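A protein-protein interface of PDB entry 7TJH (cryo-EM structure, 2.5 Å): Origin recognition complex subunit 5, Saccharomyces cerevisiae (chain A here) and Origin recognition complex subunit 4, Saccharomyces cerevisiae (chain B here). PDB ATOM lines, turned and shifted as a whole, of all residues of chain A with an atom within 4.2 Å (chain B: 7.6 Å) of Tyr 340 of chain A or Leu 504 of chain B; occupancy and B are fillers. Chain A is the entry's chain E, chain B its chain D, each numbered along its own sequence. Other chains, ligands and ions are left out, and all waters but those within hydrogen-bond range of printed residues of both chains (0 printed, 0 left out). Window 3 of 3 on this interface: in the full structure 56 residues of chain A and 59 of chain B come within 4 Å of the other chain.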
ATOM      1  N   TYR A 336      12.555  13.733  28.046  1.00  0.00           N
ATOM      2  CA  TYR A 336      13.203  13.059  26.922  1.00  0.00           C
ATOM      3  C   TYR A 336      12.870  11.569  26.903  1.00  0.00           C
ATOM      4  O   TYR A 336      12.617  10.996  25.833  1.00  0.00           O
ATOM      5  CB  TYR A 336      14.719  13.272  26.973  1.00  0.00           C
ATOM      6  CG  TYR A 336      15.397  12.964  25.656  1.00  0.00           C
ATOM      7  CD1 TYR A 336      15.555  13.948  24.689  1.00  0.00           C
ATOM      8  CD2 TYR A 336      15.853  11.680  25.369  1.00  0.00           C
ATOM      9  CE1 TYR A 336      16.155  13.665  23.478  1.00  0.00           C
ATOM     10  CE2 TYR A 336      16.445  11.386  24.163  1.00  0.00           C
ATOM     11  CZ  TYR A 336      16.595  12.381  23.223  1.00  0.00           C
ATOM     12  OH  TYR A 336      17.190  12.083  22.024  1.00  0.00           O
ATOM     13  N   ILE A 337      12.859  10.935  28.080  1.00  0.00           N
ATOM     14  CA  ILE A 337      12.485   9.522  28.174  1.00  0.00           C
ATOM     15  C   ILE A 337      11.023   9.323  27.779  1.00  0.00           C
ATOM     16  O   ILE A 337      10.692   8.422  26.998  1.00  0.00           O
ATOM     17  CB  ILE A 337      12.774   8.989  29.590  1.00  0.00           C
ATOM     18  CG1 ILE A 337      14.281   8.877  29.813  1.00  0.00           C
ATOM     19  CG2 ILE A 337      12.101   7.638  29.823  1.00  0.00           C
ATOM     20  CD1 ILE A 337      14.687   8.881  31.262  1.00  0.00           C
ATOM     21  N   CYS A 338      10.135  10.188  28.282  1.00  0.00           N
ATOM     22  CA  CYS A 338       8.710  10.104  27.962  1.00  0.00           C
ATOM     23  C   CYS A 338       8.432  10.364  26.487  1.00  0.00           C
ATOM     24  O   CYS A 338       7.468   9.825  25.933  1.00  0.00           O
ATOM     25  CB  CYS A 338       7.921  11.100  28.811  1.00  0.00           C
ATOM     26  SG  CYS A 338       7.571  10.603  30.495  1.00  0.00           S
ATOM     27  N   SER A 339       9.253  11.190  25.841  1.00  0.00           N
ATOM     28  CA  SER A 339       9.088  11.436  24.416  1.00  0.00           C
ATOM     29  C   SER A 339       9.606  10.281  23.572  1.00  0.00           C
ATOM     30  O   SER A 339       9.015   9.961  22.535  1.00  0.00           O
ATOM     31  CB  SER A 339       9.798  12.730  24.021  1.00  0.00           C
ATOM     32  OG  SER A 339       8.984  13.861  24.259  1.00  0.00           O
ATOM     33  N   TYR A 340      10.704   9.643  23.981  1.00  0.00           N
ATOM     34  CA  TYR A 340      11.379   8.695  23.103  1.00  0.00           C
ATOM     35  C   TYR A 340      11.304   7.250  23.589  1.00  0.00           C
ATOM     36  O   TYR A 340      12.056   6.404  23.101  1.00  0.00           O
ATOM     37  CB  TYR A 340      12.828   9.125  22.897  1.00  0.00           C
ATOM     38  CG  TYR A 340      12.946  10.346  22.019  1.00  0.00           C
ATOM     39  CD1 TYR A 340      12.832  10.244  20.640  1.00  0.00           C
ATOM     40  CD2 TYR A 340      13.137  11.607  22.572  1.00  0.00           C
ATOM     41  CE1 TYR A 340      12.928  11.357  19.832  1.00  0.00           C
ATOM     42  CE2 TYR A 340      13.234  12.724  21.773  1.00  0.00           C
ATOM     43  CZ  TYR A 340      13.130  12.592  20.403  1.00  0.00           C
ATOM     44  OH  TYR A 340      13.227  13.701  19.600  1.00  0.00           O
ATOM     45  N   LEU A 341      10.411   6.943  24.528  1.00  0.00           N
ATOM     46  CA  LEU A 341      10.137   5.568  24.925  1.00  0.00           C
ATOM     47  C   LEU A 341       8.635   5.352  24.983  1.00  0.00           C
ATOM     48  O   LEU A 341       7.891   6.219  25.450  1.00  0.00           O
ATOM     49  CB  LEU A 341      10.764   5.218  26.282  1.00  0.00           C
ATOM     50  CG  LEU A 341      12.271   4.968  26.331  1.00  0.00           C
ATOM     51  CD1 LEU A 341      12.691   4.508  27.716  1.00  0.00           C
ATOM     52  CD2 LEU A 341      12.679   3.948  25.285  1.00  0.00           C
ATOM     53  N   PRO A 373      14.953   5.645  17.453  1.00  0.00           N
ATOM     54  CA  PRO A 373      13.823   6.584  17.554  1.00  0.00           C
ATOM     55  C   PRO A 373      14.225   8.009  17.894  1.00  0.00           C
ATOM     56  O   PRO A 373      13.421   8.923  17.684  1.00  0.00           O
ATOM     57  CB  PRO A 373      12.960   5.969  18.662  1.00  0.00           C
ATOM     58  CG  PRO A 373      13.933   5.227  19.508  1.00  0.00           C
ATOM     59  CD  PRO A 373      14.941   4.657  18.547  1.00  0.00           C
ATOM     60  N   ARG A 374      15.439   8.234  18.398  1.00  0.00           N
ATOM     61  CA  ARG A 374      15.908   9.588  18.661  1.00  0.00           C
ATOM     62  C   ARG A 374      16.247  10.351  17.388  1.00  0.00           C
ATOM     63  O   ARG A 374      16.435  11.570  17.449  1.00  0.00           O
ATOM     64  CB  ARG A 374      17.120   9.548  19.586  1.00  0.00           C
ATOM     65  CG  ARG A 374      16.843   8.906  20.935  1.00  0.00           C
ATOM     66  CD  ARG A 374      18.135   8.559  21.639  1.00  0.00           C
ATOM     67  NE  ARG A 374      18.756   7.380  21.047  1.00  0.00           N
ATOM     68  CZ  ARG A 374      19.986   6.967  21.318  1.00  0.00           C
ATOM     69  NH1 ARG A 374      20.753   7.607  22.176  1.00  0.00           N
ATOM     70  NH2 ARG A 374      20.460   5.890  20.701  1.00  0.00           N
ATOM     71  N   TYR A 375      16.333   9.667  16.244  1.00  0.00           N
ATOM     72  CA  TYR A 375      16.454  10.340  14.958  1.00  0.00           C
ATOM     73  C   TYR A 375      15.148  10.998  14.526  1.00  0.00           C
ATOM     74  O   TYR A 375      15.177  11.931  13.718  1.00  0.00           O
ATOM     75  CB  TYR A 375      16.911   9.346  13.887  1.00  0.00           C
ATOM     76  CG  TYR A 375      18.350   8.879  14.010  1.00  0.00           C
ATOM     77  CD1 TYR A 375      19.257   9.538  14.839  1.00  0.00           C
ATOM     78  CD2 TYR A 375      18.796   7.764  13.309  1.00  0.00           C
ATOM     79  CE1 TYR A 375      20.563   9.106  14.952  1.00  0.00           C
ATOM     80  CE2 TYR A 375      20.099   7.325  13.418  1.00  0.00           C
ATOM     81  CZ  TYR A 375      20.977   7.999  14.240  1.00  0.00           C
ATOM     82  OH  TYR A 375      22.276   7.567  14.350  1.00  0.00           O
ATOM     83  N   LEU A 376      14.014  10.542  15.045  1.00  0.00           N
ATOM     84  CA  LEU A 376      12.712  11.050  14.643  1.00  0.00           C
ATOM     85  C   LEU A 376      12.231  12.149  15.589  1.00  0.00           C
ATOM     86  O   LEU A 376      12.860  12.458  16.604  1.00  0.00           O
ATOM     87  CB  LEU A 376      11.690   9.915  14.586  1.00  0.00           C
ATOM     88  CG  LEU A 376      12.099   8.680  13.782  1.00  0.00           C
ATOM     89  CD1 LEU A 376      10.996   7.640  13.784  1.00  0.00           C
ATOM     90  CD2 LEU A 376      12.484   9.064  12.357  1.00  0.00           C
ATOM     91  N   GLN A 377      11.103  12.750  15.225  1.00  0.00           N
ATOM     92  CA  GLN A 377      10.492  13.780  16.045  1.00  0.00           C
ATOM     93  C   GLN A 377       9.890  13.159  17.309  1.00  0.00           C
ATOM     94  O   GLN A 377       9.449  12.007  17.290  1.00  0.00           O
ATOM     95  CB  GLN A 377       9.422  14.523  15.242  1.00  0.00           C
ATOM     96  CG  GLN A 377       9.883  15.887  14.742  1.00  0.00           C
ATOM     97  CD  GLN A 377       8.887  16.547  13.809  1.00  0.00           C
ATOM     98  OE1 GLN A 377       8.911  16.326  12.599  1.00  0.00           O
ATOM     99  NE2 GLN A 377       8.004  17.365  14.369  1.00  0.00           N
ATOM    100  N   PRO A 378       9.888  13.892  18.425  1.00  0.00           N
ATOM    101  CA  PRO A 378       9.414  13.313  19.689  1.00  0.00           C
ATOM    102  C   PRO A 378       7.912  13.072  19.711  1.00  0.00           C
ATOM    103  O   PRO A 378       7.139  13.706  18.990  1.00  0.00           O
ATOM    104  CB  PRO A 378       9.813  14.369  20.726  1.00  0.00           C
ATOM    105  CG  PRO A 378       9.889  15.628  19.962  1.00  0.00           C
ATOM    106  CD  PRO A 378      10.445  15.241  18.632  1.00  0.00           C
ATOM    107  N   VAL A 452       9.234  16.836  24.558  1.00  0.00           N
ATOM    108  CA  VAL A 452      10.548  17.439  24.734  1.00  0.00           C
ATOM    109  C   VAL A 452      10.882  18.265  23.494  1.00  0.00           C
ATOM    110  O   VAL A 452      10.347  18.034  22.400  1.00  0.00           O
ATOM    111  CB  VAL A 452      11.615  16.360  25.027  1.00  0.00           C
ATOM    112  CG1 VAL A 452      12.090  15.656  23.752  1.00  0.00           C
ATOM    113  CG2 VAL A 452      12.799  16.941  25.797  1.00  0.00           C
ATOM    114  N   PHE A 474      18.541   3.601  26.238  1.00  0.00           N
ATOM    115  CA  PHE A 474      18.285   3.432  24.816  1.00  0.00           C
ATOM    116  C   PHE A 474      19.184   2.386  24.175  1.00  0.00           C
ATOM    117  O   PHE A 474      19.077   2.157  22.966  1.00  0.00           O
ATOM    118  CB  PHE A 474      18.453   4.771  24.084  1.00  0.00           C
ATOM    119  CG  PHE A 474      17.439   5.804  24.480  1.00  0.00           C
ATOM    120  CD1 PHE A 474      16.165   5.785  23.939  1.00  0.00           C
ATOM    121  CD2 PHE A 474      17.756   6.780  25.412  1.00  0.00           C
ATOM    122  CE1 PHE A 474      15.225   6.730  24.312  1.00  0.00           C
ATOM    123  CE2 PHE A 474      16.825   7.727  25.788  1.00  0.00           C
ATOM    124  CZ  PHE A 474      15.555   7.700  25.236  1.00  0.00           C
ATOM    125  N   PHE B 409      12.474  13.016   5.048  1.00  0.00           N
ATOM    126  CA  PHE B 409      13.750  12.718   5.689  1.00  0.00           C
ATOM    127  C   PHE B 409      14.129  13.897   6.574  1.00  0.00           C
ATOM    128  O   PHE B 409      13.558  14.984   6.471  1.00  0.00           O
ATOM    129  CB  PHE B 409      14.853  12.423   4.659  1.00  0.00           C
ATOM    130  CG  PHE B 409      15.135  13.562   3.709  1.00  0.00           C
ATOM    131  CD1 PHE B 409      14.407  13.696   2.538  1.00  0.00           C
ATOM    132  CD2 PHE B 409      16.150  14.477   3.969  1.00  0.00           C
ATOM    133  CE1 PHE B 409      14.658  14.734   1.670  1.00  0.00           C
ATOM    134  CE2 PHE B 409      16.399  15.519   3.095  1.00  0.00           C
ATOM    135  CZ  PHE B 409      15.656  15.643   1.949  1.00  0.00           C
ATOM    136  N   ASN B 410      15.114  13.673   7.442  1.00  0.00           N
ATOM    137  CA  ASN B 410      15.701  14.780   8.186  1.00  0.00           C
ATOM    138  C   ASN B 410      17.223  14.710   8.178  1.00  0.00           C
ATOM    139  O   ASN B 410      17.813  13.881   7.480  1.00  0.00           O
ATOM    140  CB  ASN B 410      15.166  14.834   9.627  1.00  0.00           C
ATOM    141  CG  ASN B 410      15.211  13.492  10.343  1.00  0.00           C
ATOM    142  OD1 ASN B 410      16.157  12.721  10.208  1.00  0.00           O
ATOM    143  ND2 ASN B 410      14.180  13.219  11.125  1.00  0.00           N
ATOM    144  N   PHE B 411      17.850  15.589   8.959  1.00  0.00           N
ATOM    145  CA  PHE B 411      19.305  15.674   9.024  1.00  0.00           C
ATOM    146  C   PHE B 411      19.920  14.423   9.649  1.00  0.00           C
ATOM    147  O   PHE B 411      20.993  13.978   9.226  1.00  0.00           O
ATOM    148  CB  PHE B 411      19.684  16.933   9.805  1.00  0.00           C
ATOM    149  CG  PHE B 411      21.153  17.144   9.961  1.00  0.00           C
ATOM    150  CD1 PHE B 411      21.911  17.624   8.908  1.00  0.00           C
ATOM    151  CD2 PHE B 411      21.776  16.892  11.175  1.00  0.00           C
ATOM    152  CE1 PHE B 411      23.264  17.831   9.052  1.00  0.00           C
ATOM    153  CE2 PHE B 411      23.132  17.094  11.326  1.00  0.00           C
ATOM    154  CZ  PHE B 411      23.878  17.566  10.262  1.00  0.00           C
ATOM    155  N   ASN B 412      19.245  13.836  10.642  1.00  0.00           N
ATOM    156  CA  ASN B 412      19.794  12.694  11.371  1.00  0.00           C
ATOM    157  C   ASN B 412      19.848  11.438  10.506  1.00  0.00           C
ATOM    158  O   ASN B 412      20.861  10.726  10.491  1.00  0.00           O
ATOM    159  CB  ASN B 412      18.966  12.442  12.630  1.00  0.00           C
ATOM    160  CG  ASN B 412      19.222  13.468  13.709  1.00  0.00           C
ATOM    161  OD1 ASN B 412      20.356  13.880  13.931  1.00  0.00           O
ATOM    162  ND2 ASN B 412      18.161  13.897  14.379  1.00  0.00           N
ATOM    163  N   GLU B 474      11.125  22.115   2.675  1.00  0.00           N
ATOM    164  CA  GLU B 474      10.422  21.723   3.892  1.00  0.00           C
ATOM    165  C   GLU B 474       9.129  21.004   3.532  1.00  0.00           C
ATOM    166  O   GLU B 474       8.466  21.351   2.552  1.00  0.00           O
ATOM    167  CB  GLU B 474      10.130  22.951   4.755  1.00  0.00           C
ATOM    168  CG  GLU B 474       9.982  22.667   6.243  1.00  0.00           C
ATOM    169  CD  GLU B 474       8.573  22.240   6.628  1.00  0.00           C
ATOM    170  OE1 GLU B 474       7.610  22.943   6.256  1.00  0.00           O
ATOM    171  OE2 GLU B 474       8.431  21.201   7.307  1.00  0.00           O
ATOM    172  N   GLY B 497       7.670  24.021  11.706  1.00  0.00           N
ATOM    173  CA  GLY B 497       9.032  23.705  11.318  1.00  0.00           C
ATOM    174  C   GLY B 497      10.064  24.626  11.936  1.00  0.00           C
ATOM    175  O   GLY B 497      11.206  24.220  12.155  1.00  0.00           O
ATOM    176  N   ILE B 500      11.040  23.704  16.080  1.00  0.00           N
ATOM    177  CA  ILE B 500      11.664  22.450  16.491  1.00  0.00           C
ATOM    178  C   ILE B 500      13.148  22.541  16.148  1.00  0.00           C
ATOM    179  O   ILE B 500      13.527  23.397  15.336  1.00  0.00           O
ATOM    180  CB  ILE B 500      10.972  21.247  15.824  1.00  0.00           C
ATOM    181  CG1 ILE B 500      11.127  21.299  14.306  1.00  0.00           C
ATOM    182  CG2 ILE B 500       9.507  21.179  16.232  1.00  0.00           C
ATOM    183  CD1 ILE B 500      10.765  20.002  13.629  1.00  0.00           C
ATOM    184  N   PRO B 501      14.027  21.742  16.772  1.00  0.00           N
ATOM    185  CA  PRO B 501      15.444  21.762  16.381  1.00  0.00           C
ATOM    186  C   PRO B 501      15.655  21.300  14.946  1.00  0.00           C
ATOM    187  O   PRO B 501      14.889  20.494  14.413  1.00  0.00           O
ATOM    188  CB  PRO B 501      16.104  20.800  17.379  1.00  0.00           C
ATOM    189  CG  PRO B 501      14.985  20.041  18.008  1.00  0.00           C
ATOM    190  CD  PRO B 501      13.828  20.978  18.015  1.00  0.00           C
ATOM    191  N   PHE B 502      16.714  21.840  14.328  1.00  0.00           N
ATOM    192  CA  PHE B 502      16.930  21.729  12.886  1.00  0.00           C
ATOM    193  C   PHE B 502      17.170  20.296  12.421  1.00  0.00           C
ATOM    194  O   PHE B 502      16.965  20.002  11.240  1.00  0.00           O
ATOM    195  CB  PHE B 502      18.109  22.618  12.462  1.00  0.00           C
ATOM    196  CG  PHE B 502      19.450  21.928  12.519  1.00  0.00           C
ATOM    197  CD1 PHE B 502      20.082  21.721  13.735  1.00  0.00           C
ATOM    198  CD2 PHE B 502      20.080  21.490  11.354  1.00  0.00           C
ATOM    199  CE1 PHE B 502      21.311  21.085  13.794  1.00  0.00           C
ATOM    200  CE2 PHE B 502      21.301  20.839  11.409  1.00  0.00           C
ATOM    201  CZ  PHE B 502      21.917  20.640  12.628  1.00  0.00           C
ATOM    202  N   ASP B 503      17.605  19.405  13.310  1.00  0.00           N
ATOM    203  CA  ASP B 503      17.899  18.031  12.929  1.00  0.00           C
ATOM    204  C   ASP B 503      16.660  17.144  12.870  1.00  0.00           C
ATOM    205  O   ASP B 503      16.774  15.979  12.479  1.00  0.00           O
ATOM    206  CB  ASP B 503      18.930  17.432  13.893  1.00  0.00           C
ATOM    207  CG  ASP B 503      18.501  17.523  15.353  1.00  0.00           C
ATOM    208  OD1 ASP B 503      17.520  18.232  15.660  1.00  0.00           O
ATOM    209  OD2 ASP B 503      19.152  16.880  16.200  1.00  0.00           O
ATOM    210  N   LEU B 504      15.490  17.661  13.239  1.00  0.00           N
ATOM    211  CA  LEU B 504      14.243  16.915  13.157  1.00  0.00           C
ATOM    212  C   LEU B 504      13.267  17.493  12.142  1.00  0.00           C
ATOM    213  O   LEU B 504      12.143  16.994  12.035  1.00  0.00           O
ATOM    214  CB  LEU B 504      13.572  16.852  14.534  1.00  0.00           C
ATOM    215  CG  LEU B 504      14.433  16.342  15.689  1.00  0.00           C
ATOM    216  CD1 LEU B 504      13.656  16.394  16.987  1.00  0.00           C
ATOM    217  CD2 LEU B 504      14.928  14.933  15.411  1.00  0.00           C
ATOM    218  N   ARG B 505      13.659  18.530  11.405  1.00  0.00           N
ATOM    219  CA  ARG B 505      12.787  19.114  10.394  1.00  0.00           C
ATOM    220  C   ARG B 505      12.645  18.173   9.205  1.00  0.00           C
ATOM    221  O   ARG B 505      13.637  17.643   8.698  1.00  0.00           O
ATOM    222  CB  ARG B 505      13.338  20.462   9.933  1.00  0.00           C
ATOM    223  CG  ARG B 505      13.167  21.583  10.931  1.00  0.00           C
ATOM    224  CD  ARG B 505      13.580  22.916  10.333  1.00  0.00           C
ATOM    225  NE  ARG B 505      14.180  23.793  11.332  1.00  0.00           N
ATOM    226  CZ  ARG B 505      15.225  24.578  11.109  1.00  0.00           C
ATOM    227  NH1 ARG B 505      15.796  24.648   9.918  1.00  0.00           N
ATOM    228  NH2 ARG B 505      15.706  25.316  12.105  1.00  0.00           N
ATOM    229  N   SER B 506      11.410  17.970   8.758  1.00  0.00           N
ATOM    230  CA  SER B 506      11.141  17.068   7.648  1.00  0.00           C
ATOM    231  C   SER B 506      11.344  17.781   6.317  1.00  0.00           C
ATOM    232  O   SER B 506      10.867  18.905   6.122  1.00  0.00           O
ATOM    233  CB  SER B 506       9.720  16.522   7.748  1.00  0.00           C
ATOM    234  OG  SER B 506       9.656  15.460   8.677  1.00  0.00           O
ATOM    235  N   TYR B 507      12.045  17.122   5.398  1.00  0.00           N
ATOM    236  CA  TYR B 507      12.335  17.674   4.085  1.00  0.00           C
ATOM    237  C   TYR B 507      11.991  16.662   3.005  1.00  0.00           C
ATOM    238  O   TYR B 507      11.842  15.468   3.261  1.00  0.00           O
ATOM    239  CB  TYR B 507      13.808  18.077   3.940  1.00  0.00           C
ATOM    240  CG  TYR B 507      14.199  19.302   4.721  1.00  0.00           C
ATOM    241  CD1 TYR B 507      13.938  20.577   4.231  1.00  0.00           C
ATOM    242  CD2 TYR B 507      14.835  19.187   5.950  1.00  0.00           C
ATOM    243  CE1 TYR B 507      14.295  21.703   4.949  1.00  0.00           C
ATOM    244  CE2 TYR B 507      15.197  20.302   6.672  1.00  0.00           C
ATOM    245  CZ  TYR B 507      14.926  21.557   6.168  1.00  0.00           C
ATOM    246  OH  TYR B 507      15.294  22.664   6.889  1.00  0.00           O
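Tyr 336 of chain A touches none of the printed residues of chain B.
Tyr 340 of chain A touches just one residue of chain B: Leu 504.
Of the printed residues of chain B, Tyr 375 of chain A touches Asn 410 (3.1 Å), Asn 412 (3.6 Å) and Leu 504 (3.5 Å).
Printed residues of chain B within 4 Å of Leu 376 of chain A: Leu 504.
Of the printed residues of chain A, Asn 410 of chain B touches Tyr 375.
Printed residues of chain A within 4 Å of Asn 412 of chain B: Tyr 375 (3.6 Å).
Leu 504 of chain B touches five residues of chain A.
The nearest printed residue of chain B that does not touch Pro 378 of chain A is Ile 500 of chain B (6.5 Å).
N of Asn 412 of chain B lies close to OD1 of Asn 410 of chain B (3.3 Å).
O of Asp 503 of chain B lies within hydrogen-bond range of ND2 of Asn 412 of chain B (3.1 Å).
The side-chain hydroxyl (OH) of Tyr 340 of chain A lies within hydrogen-bond range of the backbone carbonyl oxygen (O) of Leu 376 of chain A.
Of the 14 printed residues of chain B, 4 touch a printed residue of chain A.
Hydrophobic or aromatic side chains of chain A that line the printed part of chain B: Tyr 340, Tyr 375 and Pro 378.
Among the printed residues, no Asp or Glu carboxylate lies within 4 Å of a Lys or Arg side-chain nitrogen of the other chain.
ND2 of Asn 410 of chain B is in hydrogen-bond range of O of Tyr 375 of chain A.
The side-chain amide oxygen (OE1) of Gln 377 of chain A sits close to the backbone carbonyl oxygen (O) of Leu 504 of chain B, at 3.3 Å.
Tyr 340 of chain A touches Leu 504 of chain B.
Asn 412 of chain B touches Tyr 375 of chain A (ND2 to O, 3.6 Å).
O of Tyr 375 of chain A touches CD2 of Leu 504 of chain B, at 3.5 Å.
O of Leu 376 of chain A touches CD2 of Leu 504 of chain B (3.4 Å).
Gln 377 of chain A touches Ile 500 of chain B (NE2 to CD1, 3.9 Å).
CD of Pro 378 of chain A touches CD1 of Leu 504 of chain B, 3.8 Å away.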
